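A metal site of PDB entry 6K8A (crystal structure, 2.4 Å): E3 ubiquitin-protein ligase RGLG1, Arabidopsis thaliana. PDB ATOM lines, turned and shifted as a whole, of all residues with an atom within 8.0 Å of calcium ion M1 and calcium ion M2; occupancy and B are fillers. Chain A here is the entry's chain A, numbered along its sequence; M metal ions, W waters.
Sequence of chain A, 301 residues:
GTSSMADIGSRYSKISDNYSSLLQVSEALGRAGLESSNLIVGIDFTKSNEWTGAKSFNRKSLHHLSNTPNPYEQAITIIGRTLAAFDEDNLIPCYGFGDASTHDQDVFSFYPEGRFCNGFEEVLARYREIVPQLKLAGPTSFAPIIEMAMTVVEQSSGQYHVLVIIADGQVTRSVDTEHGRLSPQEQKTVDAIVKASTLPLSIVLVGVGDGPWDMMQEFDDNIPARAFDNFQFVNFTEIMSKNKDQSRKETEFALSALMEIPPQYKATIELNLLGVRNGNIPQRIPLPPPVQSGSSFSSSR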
ATOM      1  N   SER A  13      32.396 -17.123   9.321  1.00  0.00           N
ATOM      2  CA  SER A  13      33.146 -18.369   9.261  1.00  0.00           C
ATOM      3  C   SER A  13      32.563 -19.375  10.278  1.00  0.00           C
ATOM      4  O   SER A  13      32.002 -18.958  11.286  1.00  0.00           O
ATOM      5  CB  SER A  13      34.637 -18.106   9.528  1.00  0.00           C
ATOM      6  OG  SER A  13      35.410 -19.309   9.422  1.00  0.00           O
ATOM      7  N   LYS A  14      32.712 -20.672  10.002  1.00  0.00           N
ATOM      8  CA  LYS A  14      32.123 -21.736  10.837  1.00  0.00           C
ATOM      9  C   LYS A  14      32.949 -22.012  12.098  1.00  0.00           C
ATOM     10  O   LYS A  14      34.165 -21.981  12.057  1.00  0.00           O
ATOM     11  CB  LYS A  14      31.978 -23.041  10.032  1.00  0.00           C
ATOM     12  CG  LYS A  14      31.136 -24.132  10.739  1.00  0.00           C
ATOM     13  CD  LYS A  14      31.473 -25.572  10.263  1.00  0.00           C
ATOM     14  CE  LYS A  14      32.876 -26.006  10.681  1.00  0.00           C
ATOM     15  NZ  LYS A  14      32.900 -27.402  11.252  1.00  0.00           N
ATOM     16  N   ILE A  15      32.257 -22.291  13.208  1.00  0.00           N
ATOM     17  CA  ILE A  15      32.926 -22.541  14.483  1.00  0.00           C
ATOM     18  C   ILE A  15      32.887 -24.009  14.830  1.00  0.00           C
ATOM     19  O   ILE A  15      31.808 -24.565  15.067  1.00  0.00           O
ATOM     20  CB  ILE A  15      32.286 -21.739  15.635  1.00  0.00           C
ATOM     21  CG1 ILE A  15      32.411 -20.225  15.383  1.00  0.00           C
ATOM     22  CG2 ILE A  15      32.926 -22.103  16.969  1.00  0.00           C
ATOM     23  CD1 ILE A  15      31.751 -19.406  16.452  1.00  0.00           C
ATOM     24  N   SER A  16      34.066 -24.636  14.882  1.00  0.00           N
ATOM     25  CA  SER A  16      34.161 -26.073  15.182  1.00  0.00           C
ATOM     26  C   SER A  16      34.157 -26.330  16.682  1.00  0.00           C
ATOM     27  O   SER A  16      34.143 -25.392  17.477  1.00  0.00           O
ATOM     28  CB  SER A  16      35.423 -26.642  14.545  1.00  0.00           C
ATOM     29  OG  SER A  16      35.483 -26.325  13.170  1.00  0.00           O
ATOM     30  N   ASP A  17      34.153 -27.608  17.055  1.00  0.00           N
ATOM     31  CA  ASP A  17      34.276 -28.014  18.461  1.00  0.00           C
ATOM     32  C   ASP A  17      35.730 -27.904  18.892  1.00  0.00           C
ATOM     33  O   ASP A  17      36.496 -28.854  18.749  1.00  0.00           O
ATOM     34  CB  ASP A  17      33.781 -29.450  18.675  1.00  0.00           C
ATOM     35  CG  ASP A  17      32.266 -29.597  18.511  1.00  0.00           C
ATOM     36  OD1 ASP A  17      31.557 -28.595  18.266  1.00  0.00           O
ATOM     37  OD2 ASP A  17      31.786 -30.736  18.641  1.00  0.00           O
ATOM     38  N   ILE A 203      23.004 -18.040  19.894  1.00  0.00           N
ATOM     39  CA  ILE A 203      21.838 -18.931  19.910  1.00  0.00           C
ATOM     40  C   ILE A 203      22.266 -20.377  20.209  1.00  0.00           C
ATOM     41  O   ILE A 203      23.200 -20.905  19.584  1.00  0.00           O
ATOM     42  CB  ILE A 203      21.075 -18.884  18.567  1.00  0.00           C
ATOM     43  CG1 ILE A 203      20.664 -17.431  18.242  1.00  0.00           C
ATOM     44  CG2 ILE A 203      19.873 -19.784  18.624  1.00  0.00           C
ATOM     45  CD1 ILE A 203      20.287 -17.207  16.812  1.00  0.00           C
ATOM     46  N   MET A 216      18.549 -28.712  12.119  1.00  0.00           N
ATOM     47  CA  MET A 216      19.232 -28.042  13.214  1.00  0.00           C
ATOM     48  C   MET A 216      20.727 -28.031  12.970  1.00  0.00           C
ATOM     49  O   MET A 216      21.399 -27.037  13.252  1.00  0.00           O
ATOM     50  CB  MET A 216      18.916 -28.703  14.540  1.00  0.00           C
ATOM     51  CG  MET A 216      17.435 -28.644  14.937  1.00  0.00           C
ATOM     52  SD  MET A 216      16.661 -27.002  14.839  1.00  0.00           S
ATOM     53  CE  MET A 216      15.995 -26.968  13.179  1.00  0.00           C
ATOM     54  N   GLN A 217      21.266 -29.115  12.415  1.00  0.00           N
ATOM     55  CA  GLN A 217      22.697 -29.162  12.127  1.00  0.00           C
ATOM     56  C   GLN A 217      23.036 -28.185  11.019  1.00  0.00           C
ATOM     57  O   GLN A 217      24.125 -27.586  11.020  1.00  0.00           O
ATOM     58  CB  GLN A 217      23.138 -30.585  11.776  1.00  0.00           C
ATOM     59  CG  GLN A 217      23.130 -31.509  12.997  1.00  0.00           C
ATOM     60  CD  GLN A 217      23.229 -32.989  12.647  1.00  0.00           C
ATOM     61  OE1 GLN A 217      23.009 -33.393  11.501  1.00  0.00           O
ATOM     62  NE2 GLN A 217      23.549 -33.818  13.657  1.00  0.00           N
ATOM     63  N   GLU A 218      22.110 -27.982  10.088  1.00  0.00           N
ATOM     64  CA  GLU A 218      22.350 -27.000   9.038  1.00  0.00           C
ATOM     65  C   GLU A 218      22.324 -25.572   9.590  1.00  0.00           C
ATOM     66  O   GLU A 218      23.035 -24.711   9.080  1.00  0.00           O
ATOM     67  CB  GLU A 218      21.331 -27.158   7.918  1.00  0.00           C
ATOM     68  CG  GLU A 218      21.909 -27.884   6.706  1.00  0.00           C
ATOM     69  CD  GLU A 218      21.614 -27.166   5.380  1.00  0.00           C
ATOM     70  OE1 GLU A 218      21.185 -25.974   5.393  1.00  0.00           O
ATOM     71  OE2 GLU A 218      21.819 -27.814   4.322  1.00  0.00           O
ATOM     72  N   PHE A 219      21.525 -25.307  10.622  1.00  0.00           N
ATOM     73  CA  PHE A 219      21.530 -23.983  11.234  1.00  0.00           C
ATOM     74  C   PHE A 219      22.845 -23.769  11.961  1.00  0.00           C
ATOM     75  O   PHE A 219      23.394 -22.667  11.977  1.00  0.00           O
ATOM     76  CB  PHE A 219      20.383 -23.801  12.234  1.00  0.00           C
ATOM     77  CG  PHE A 219      19.039 -23.726  11.610  1.00  0.00           C
ATOM     78  CD1 PHE A 219      18.903 -23.608  10.235  1.00  0.00           C
ATOM     79  CD2 PHE A 219      17.906 -23.812  12.393  1.00  0.00           C
ATOM     80  CE1 PHE A 219      17.648 -23.564   9.657  1.00  0.00           C
ATOM     81  CE2 PHE A 219      16.651 -23.767  11.815  1.00  0.00           C
ATOM     82  CZ  PHE A 219      16.527 -23.624  10.454  1.00  0.00           C
ATOM     83  N   ASP A 220      23.327 -24.853  12.573  1.00  0.00           N
ATOM     84  CA  ASP A 220      24.565 -24.873  13.325  1.00  0.00           C
ATOM     85  C   ASP A 220      25.750 -24.578  12.413  1.00  0.00           C
ATOM     86  O   ASP A 220      26.575 -23.736  12.719  1.00  0.00           O
ATOM     87  CB  ASP A 220      24.708 -26.236  14.015  1.00  0.00           C
ATOM     88  CG  ASP A 220      25.913 -26.351  14.930  1.00  0.00           C
ATOM     89  OD1 ASP A 220      26.568 -25.332  15.205  1.00  0.00           O
ATOM     90  OD2 ASP A 220      26.197 -27.471  15.394  1.00  0.00           O
ATOM     91  N   ASP A 221      25.802 -25.240  11.255  1.00  0.00           N
ATOM     92  CA  ASP A 221      27.033 -25.290  10.473  1.00  0.00           C
ATOM     93  C   ASP A 221      26.999 -24.590   9.118  1.00  0.00           C
ATOM     94  O   ASP A 221      28.051 -24.336   8.543  1.00  0.00           O
ATOM     95  CB  ASP A 221      27.445 -26.750  10.220  1.00  0.00           C
ATOM     96  CG  ASP A 221      27.667 -27.557  11.502  1.00  0.00           C
ATOM     97  OD1 ASP A 221      28.304 -27.020  12.447  1.00  0.00           O
ATOM     98  OD2 ASP A 221      27.200 -28.725  11.552  1.00  0.00           O
ATOM     99  N   ASN A 222      25.823 -24.313   8.570  1.00  0.00           N
ATOM    100  CA  ASN A 222      25.802 -23.890   7.170  1.00  0.00           C
ATOM    101  C   ASN A 222      24.745 -22.840   6.779  1.00  0.00           C
ATOM    102  O   ASN A 222      23.713 -23.179   6.188  1.00  0.00           O
ATOM    103  CB  ASN A 222      25.633 -25.128   6.288  1.00  0.00           C
ATOM    104  CG  ASN A 222      25.813 -24.809   4.819  1.00  0.00           C
ATOM    105  OD1 ASN A 222      26.697 -24.027   4.443  1.00  0.00           O
ATOM    106  ND2 ASN A 222      24.959 -25.406   3.977  1.00  0.00           N
ATOM    107  N   ARG A 226      25.189 -15.200   6.980  1.00  0.00           N
ATOM    108  CA  ARG A 226      25.279 -14.549   8.279  1.00  0.00           C
ATOM    109  C   ARG A 226      26.692 -13.982   8.543  1.00  0.00           C
ATOM    110  O   ARG A 226      27.668 -14.421   7.941  1.00  0.00           O
ATOM    111  CB  ARG A 226      24.856 -15.510   9.397  1.00  0.00           C
ATOM    112  CG  ARG A 226      25.651 -16.771   9.451  1.00  0.00           C
ATOM    113  CD  ARG A 226      25.285 -17.596  10.670  1.00  0.00           C
ATOM    114  NE  ARG A 226      25.882 -18.920  10.588  1.00  0.00           N
ATOM    115  CZ  ARG A 226      25.464 -19.979  11.274  1.00  0.00           C
ATOM    116  NH1 ARG A 226      24.440 -19.859  12.120  1.00  0.00           N
ATOM    117  NH2 ARG A 226      26.066 -21.145  11.111  1.00  0.00           N
ATOM    118  N   PHE A 228      28.550 -14.040  11.248  1.00  0.00           N
ATOM    119  CA  PHE A 228      29.383 -14.988  11.977  1.00  0.00           C
ATOM    120  C   PHE A 228      28.523 -16.162  12.425  1.00  0.00           C
ATOM    121  O   PHE A 228      27.297 -16.069  12.488  1.00  0.00           O
ATOM    122  CB  PHE A 228      30.038 -14.333  13.180  1.00  0.00           C
ATOM    123  CG  PHE A 228      29.081 -13.983  14.298  1.00  0.00           C
ATOM    124  CD1 PHE A 228      28.301 -12.828  14.244  1.00  0.00           C
ATOM    125  CD2 PHE A 228      28.982 -14.818  15.426  1.00  0.00           C
ATOM    126  CE1 PHE A 228      27.425 -12.489  15.275  1.00  0.00           C
ATOM    127  CE2 PHE A 228      28.108 -14.493  16.459  1.00  0.00           C
ATOM    128  CZ  PHE A 228      27.330 -13.311  16.383  1.00  0.00           C
ATOM    129  N   ASP A 229      29.172 -17.272  12.748  1.00  0.00           N
ATOM    130  CA  ASP A 229      28.482 -18.470  13.187  1.00  0.00           C
ATOM    131  C   ASP A 229      27.877 -18.220  14.572  1.00  0.00           C
ATOM    132  O   ASP A 229      28.573 -18.328  15.593  1.00  0.00           O
ATOM    133  CB  ASP A 229      29.444 -19.659  13.184  1.00  0.00           C
ATOM    134  CG  ASP A 229      28.764 -20.957  13.610  1.00  0.00           C
ATOM    135  OD1 ASP A 229      27.585 -20.922  13.994  1.00  0.00           O
ATOM    136  OD2 ASP A 229      29.447 -22.008  13.579  1.00  0.00           O
ATOM    137  N   ASN A 230      26.580 -17.905  14.598  1.00  0.00           N
ATOM    138  CA  ASN A 230      25.895 -17.485  15.816  1.00  0.00           C
ATOM    139  C   ASN A 230      24.973 -18.543  16.427  1.00  0.00           C
ATOM    140  O   ASN A 230      24.162 -18.240  17.302  1.00  0.00           O
ATOM    141  CB  ASN A 230      25.070 -16.233  15.536  1.00  0.00           C
ATOM    142  CG  ASN A 230      23.984 -16.481  14.480  1.00  0.00           C
ATOM    143  OD1 ASN A 230      23.886 -17.577  13.929  1.00  0.00           O
ATOM    144  ND2 ASN A 230      23.181 -15.458  14.187  1.00  0.00           N
ATOM    145  N   PHE A 231      25.111 -19.784  15.962  1.00  0.00           N
ATOM    146  CA  PHE A 231      24.141 -20.834  16.265  1.00  0.00           C
ATOM    147  C   PHE A 231      24.804 -22.159  16.647  1.00  0.00           C
ATOM    148  O   PHE A 231      25.606 -22.696  15.887  1.00  0.00           O
ATOM    149  CB  PHE A 231      23.232 -21.057  15.050  1.00  0.00           C
ATOM    150  CG  PHE A 231      21.977 -21.837  15.349  1.00  0.00           C
ATOM    151  CD1 PHE A 231      21.998 -23.222  15.447  1.00  0.00           C
ATOM    152  CD2 PHE A 231      20.758 -21.186  15.495  1.00  0.00           C
ATOM    153  CE1 PHE A 231      20.831 -23.942  15.701  1.00  0.00           C
ATOM    154  CE2 PHE A 231      19.583 -21.901  15.746  1.00  0.00           C
ATOM    155  CZ  PHE A 231      19.625 -23.289  15.852  1.00  0.00           C
ATOM    156  N   GLN A 232      24.462 -22.676  17.817  1.00  0.00           N
ATOM    157  CA  GLN A 232      24.945 -23.976  18.237  1.00  0.00           C
ATOM    158  C   GLN A 232      23.781 -24.936  18.472  1.00  0.00           C
ATOM    159  O   GLN A 232      22.753 -24.566  19.048  1.00  0.00           O
ATOM    160  CB  GLN A 232      25.799 -23.873  19.501  1.00  0.00           C
ATOM    161  CG  GLN A 232      26.052 -25.192  20.219  1.00  0.00           C
ATOM    162  CD  GLN A 232      26.998 -26.128  19.480  1.00  0.00           C
ATOM    163  OE1 GLN A 232      27.036 -26.175  18.243  1.00  0.00           O
ATOM    164  NE2 GLN A 232      27.772 -26.888  20.241  1.00  0.00           N
ATOM    165  N   PHE A 233      23.952 -26.168  17.977  1.00  0.00           N
ATOM    166  CA  PHE A 233      23.008 -27.249  18.227  1.00  0.00           C
ATOM    167  C   PHE A 233      23.521 -28.244  19.264  1.00  0.00           C
ATOM    168  O   PHE A 233      24.596 -28.820  19.092  1.00  0.00           O
ATOM    169  CB  PHE A 233      22.700 -27.987  16.924  1.00  0.00           C
ATOM    170  CG  PHE A 233      21.914 -29.243  17.115  1.00  0.00           C
ATOM    171  CD1 PHE A 233      20.707 -29.228  17.811  1.00  0.00           C
ATOM    172  CD2 PHE A 233      22.372 -30.451  16.599  1.00  0.00           C
ATOM    173  CE1 PHE A 233      19.968 -30.381  18.003  1.00  0.00           C
ATOM    174  CE2 PHE A 233      21.634 -31.627  16.782  1.00  0.00           C
ATOM    175  CZ  PHE A 233      20.438 -31.596  17.481  1.00  0.00           C
ATOM    176  N   VAL A 234      22.746 -28.411  20.327  1.00  0.00           N
ATOM    177  CA  VAL A 234      22.984 -29.418  21.346  1.00  0.00           C
ATOM    178  C   VAL A 234      21.957 -30.550  21.267  1.00  0.00           C
ATOM    179  O   VAL A 234      20.782 -30.334  21.580  1.00  0.00           O
ATOM    180  CB  VAL A 234      22.914 -28.831  22.758  1.00  0.00           C
ATOM    181  CG1 VAL A 234      23.037 -29.940  23.813  1.00  0.00           C
ATOM    182  CG2 VAL A 234      23.975 -27.768  22.950  1.00  0.00           C
ATOM    183  N   SER A 256      28.729 -28.884  25.505  1.00  0.00           N
ATOM    184  CA  SER A 256      28.087 -28.719  24.202  1.00  0.00           C
ATOM    185  C   SER A 256      27.441 -27.329  24.048  1.00  0.00           C
ATOM    186  O   SER A 256      27.582 -26.686  23.020  1.00  0.00           O
ATOM    187  CB  SER A 256      27.019 -29.794  23.976  1.00  0.00           C
ATOM    188  OG  SER A 256      27.566 -31.080  24.173  1.00  0.00           O
ATOM    189  N   MET A 259      30.183 -24.569  23.769  1.00  0.00           N
ATOM    190  CA  MET A 259      31.240 -24.842  22.793  1.00  0.00           C
ATOM    191  C   MET A 259      31.581 -23.645  21.910  1.00  0.00           C
ATOM    192  O   MET A 259      32.761 -23.369  21.661  1.00  0.00           O
ATOM    193  CB  MET A 259      30.843 -26.026  21.896  1.00  0.00           C
ATOM    194  CG  MET A 259      31.973 -26.517  20.991  1.00  0.00           C
ATOM    195  SD  MET A 259      33.359 -27.226  21.940  1.00  0.00           S
ATOM    196  CE  MET A 259      32.619 -28.783  22.463  1.00  0.00           C
ATOM    197  N   GLU A 260      30.566 -22.944  21.435  1.00  0.00           N
ATOM    198  CA  GLU A 260      30.798 -21.857  20.495  1.00  0.00           C
ATOM    199  C   GLU A 260      30.770 -20.483  21.145  1.00  0.00           C
ATOM    200  O   GLU A 260      30.980 -19.471  20.468  1.00  0.00           O
ATOM    201  CB  GLU A 260      29.779 -21.916  19.359  1.00  0.00           C
ATOM    202  CG  GLU A 260      29.754 -23.251  18.622  1.00  0.00           C
ATOM    203  CD  GLU A 260      28.921 -23.195  17.337  1.00  0.00           C
ATOM    204  OE1 GLU A 260      28.604 -22.079  16.883  1.00  0.00           O
ATOM    205  OE2 GLU A 260      28.604 -24.255  16.776  1.00  0.00           O
ATOM    206  N   GLN A 264      32.084 -16.759  19.684  1.00  0.00           N
ATOM    207  CA  GLN A 264      30.932 -15.895  19.385  1.00  0.00           C
ATOM    208  C   GLN A 264      31.059 -14.583  20.151  1.00  0.00           C
ATOM    209  O   GLN A 264      30.851 -13.505  19.590  1.00  0.00           O
ATOM    210  CB  GLN A 264      29.619 -16.595  19.711  1.00  0.00           C
ATOM    211  CG  GLN A 264      29.134 -17.499  18.606  1.00  0.00           C
ATOM    212  CD  GLN A 264      28.012 -18.421  19.059  1.00  0.00           C
ATOM    213  OE1 GLN A 264      27.599 -18.372  20.227  1.00  0.00           O
ATOM    214  NE2 GLN A 264      27.519 -19.275  18.152  1.00  0.00           N
HETATM  215 CA    CA M   1      28.427 -26.627  16.407  1.00  0.00          CA
HETATM  216 CA    CA M   2      27.617 -23.173  14.835  1.00  0.00          CA
HETATM  217  O   HOH W   1      28.917 -28.174  14.752  1.00  0.00           O
HETATM  218  O   HOH W   2      29.095 -24.963  13.987  1.00  0.00           O
HETATM  219  O   HOH W   3      30.810 -26.216  16.857  1.00  0.00           O
HETATM  220  O   HOH W   4      28.768 -28.467  17.945  1.00  0.00           O
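The side-chain amide nitrogen (NE2) of Gln 264 is in hydrogen-bond range of the backbone carbonyl oxygen (O) of Asp 229 (2.9 Å). The backbone NH (N) of Phe 231 sits close to the side-chain amide nitrogen (NE2) of Gln 264 (3.3 Å). The side-chain carboxylate (OE1) of Glu 260 sits close to the side-chain amide nitrogen (NE2) of Gln 264 (3.3 Å). The backbone NH (N) of Ile 15 lies close to the side-chain carboxylate (OD2) of Asp 229 (2.8 Å). The side-chain amide nitrogen of Gln 232 sits at hydrogen-bond distance from the backbone carbonyl oxygen of Ser 256 (2.8 Å). The backbone NH (N) of Gln 232 is in hydrogen-bond range of the backbone carbonyl oxygen (O) of Ile 203 (2.8 Å). O of Asp 220 sits close to NH2 of Arg 226 (3.1 Å). The guanidinium group (NH2) of Arg 226 sits close to the side-chain carboxylate (OD1) of Asp 229, at 3.3 Å.
Of the 25 residues printed, 4 come within 4 Å of calcium ion M2. The nearest printed residue that does not touch calcium ion M2 is Gln 232 (4.4 Å).
Water W4 lies within hydrogen-bond range of the side-chain carboxylate of Asp 17 (2.8 Å) and the side-chain amide nitrogen of Gln 232 (3.0 Å). Water W2 bridges the side-chain carboxylate (OD1) of Asp 221 (2.7 Å) and the backbone carbonyl oxygen (O) of Ile 15 (2.9 Å).
Merely in contact with calcium ion M1: Asp 221 (3.98 Å). Within 4 Å of calcium ion M1: Asp 220, Asp 221, Gln 232 and Glu 260.
Calcium ion M1 is bound by water W1 (2.3 Å), OE1 of Gln 232 (2.3 Å), OE2 of Glu 260 (2.4 Å), water W4 (2.4 Å), water W3 (2.5 Å), OD1 of Asp 220 (2.6 Å) and OD2 of Asp 220 (2.6 Å). Slightly farther from calcium ion M1 lies water W2 (3.0 Å).
Calcium ion M2 is bound by the backbone carbonyl oxygen (O) of Phe 231, the side-chain carboxylate (OD1) of Asp 229, the backbone carbonyl oxygen (O) of Asp 220, the side-chain carboxylate (OD1) of Asp 220, the side-chain carboxylate (OE2) of Glu 260, water W2, the side-chain carboxylate (OD2) of Asp 229 and the side-chain carboxylate (OE1) of Glu 260.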
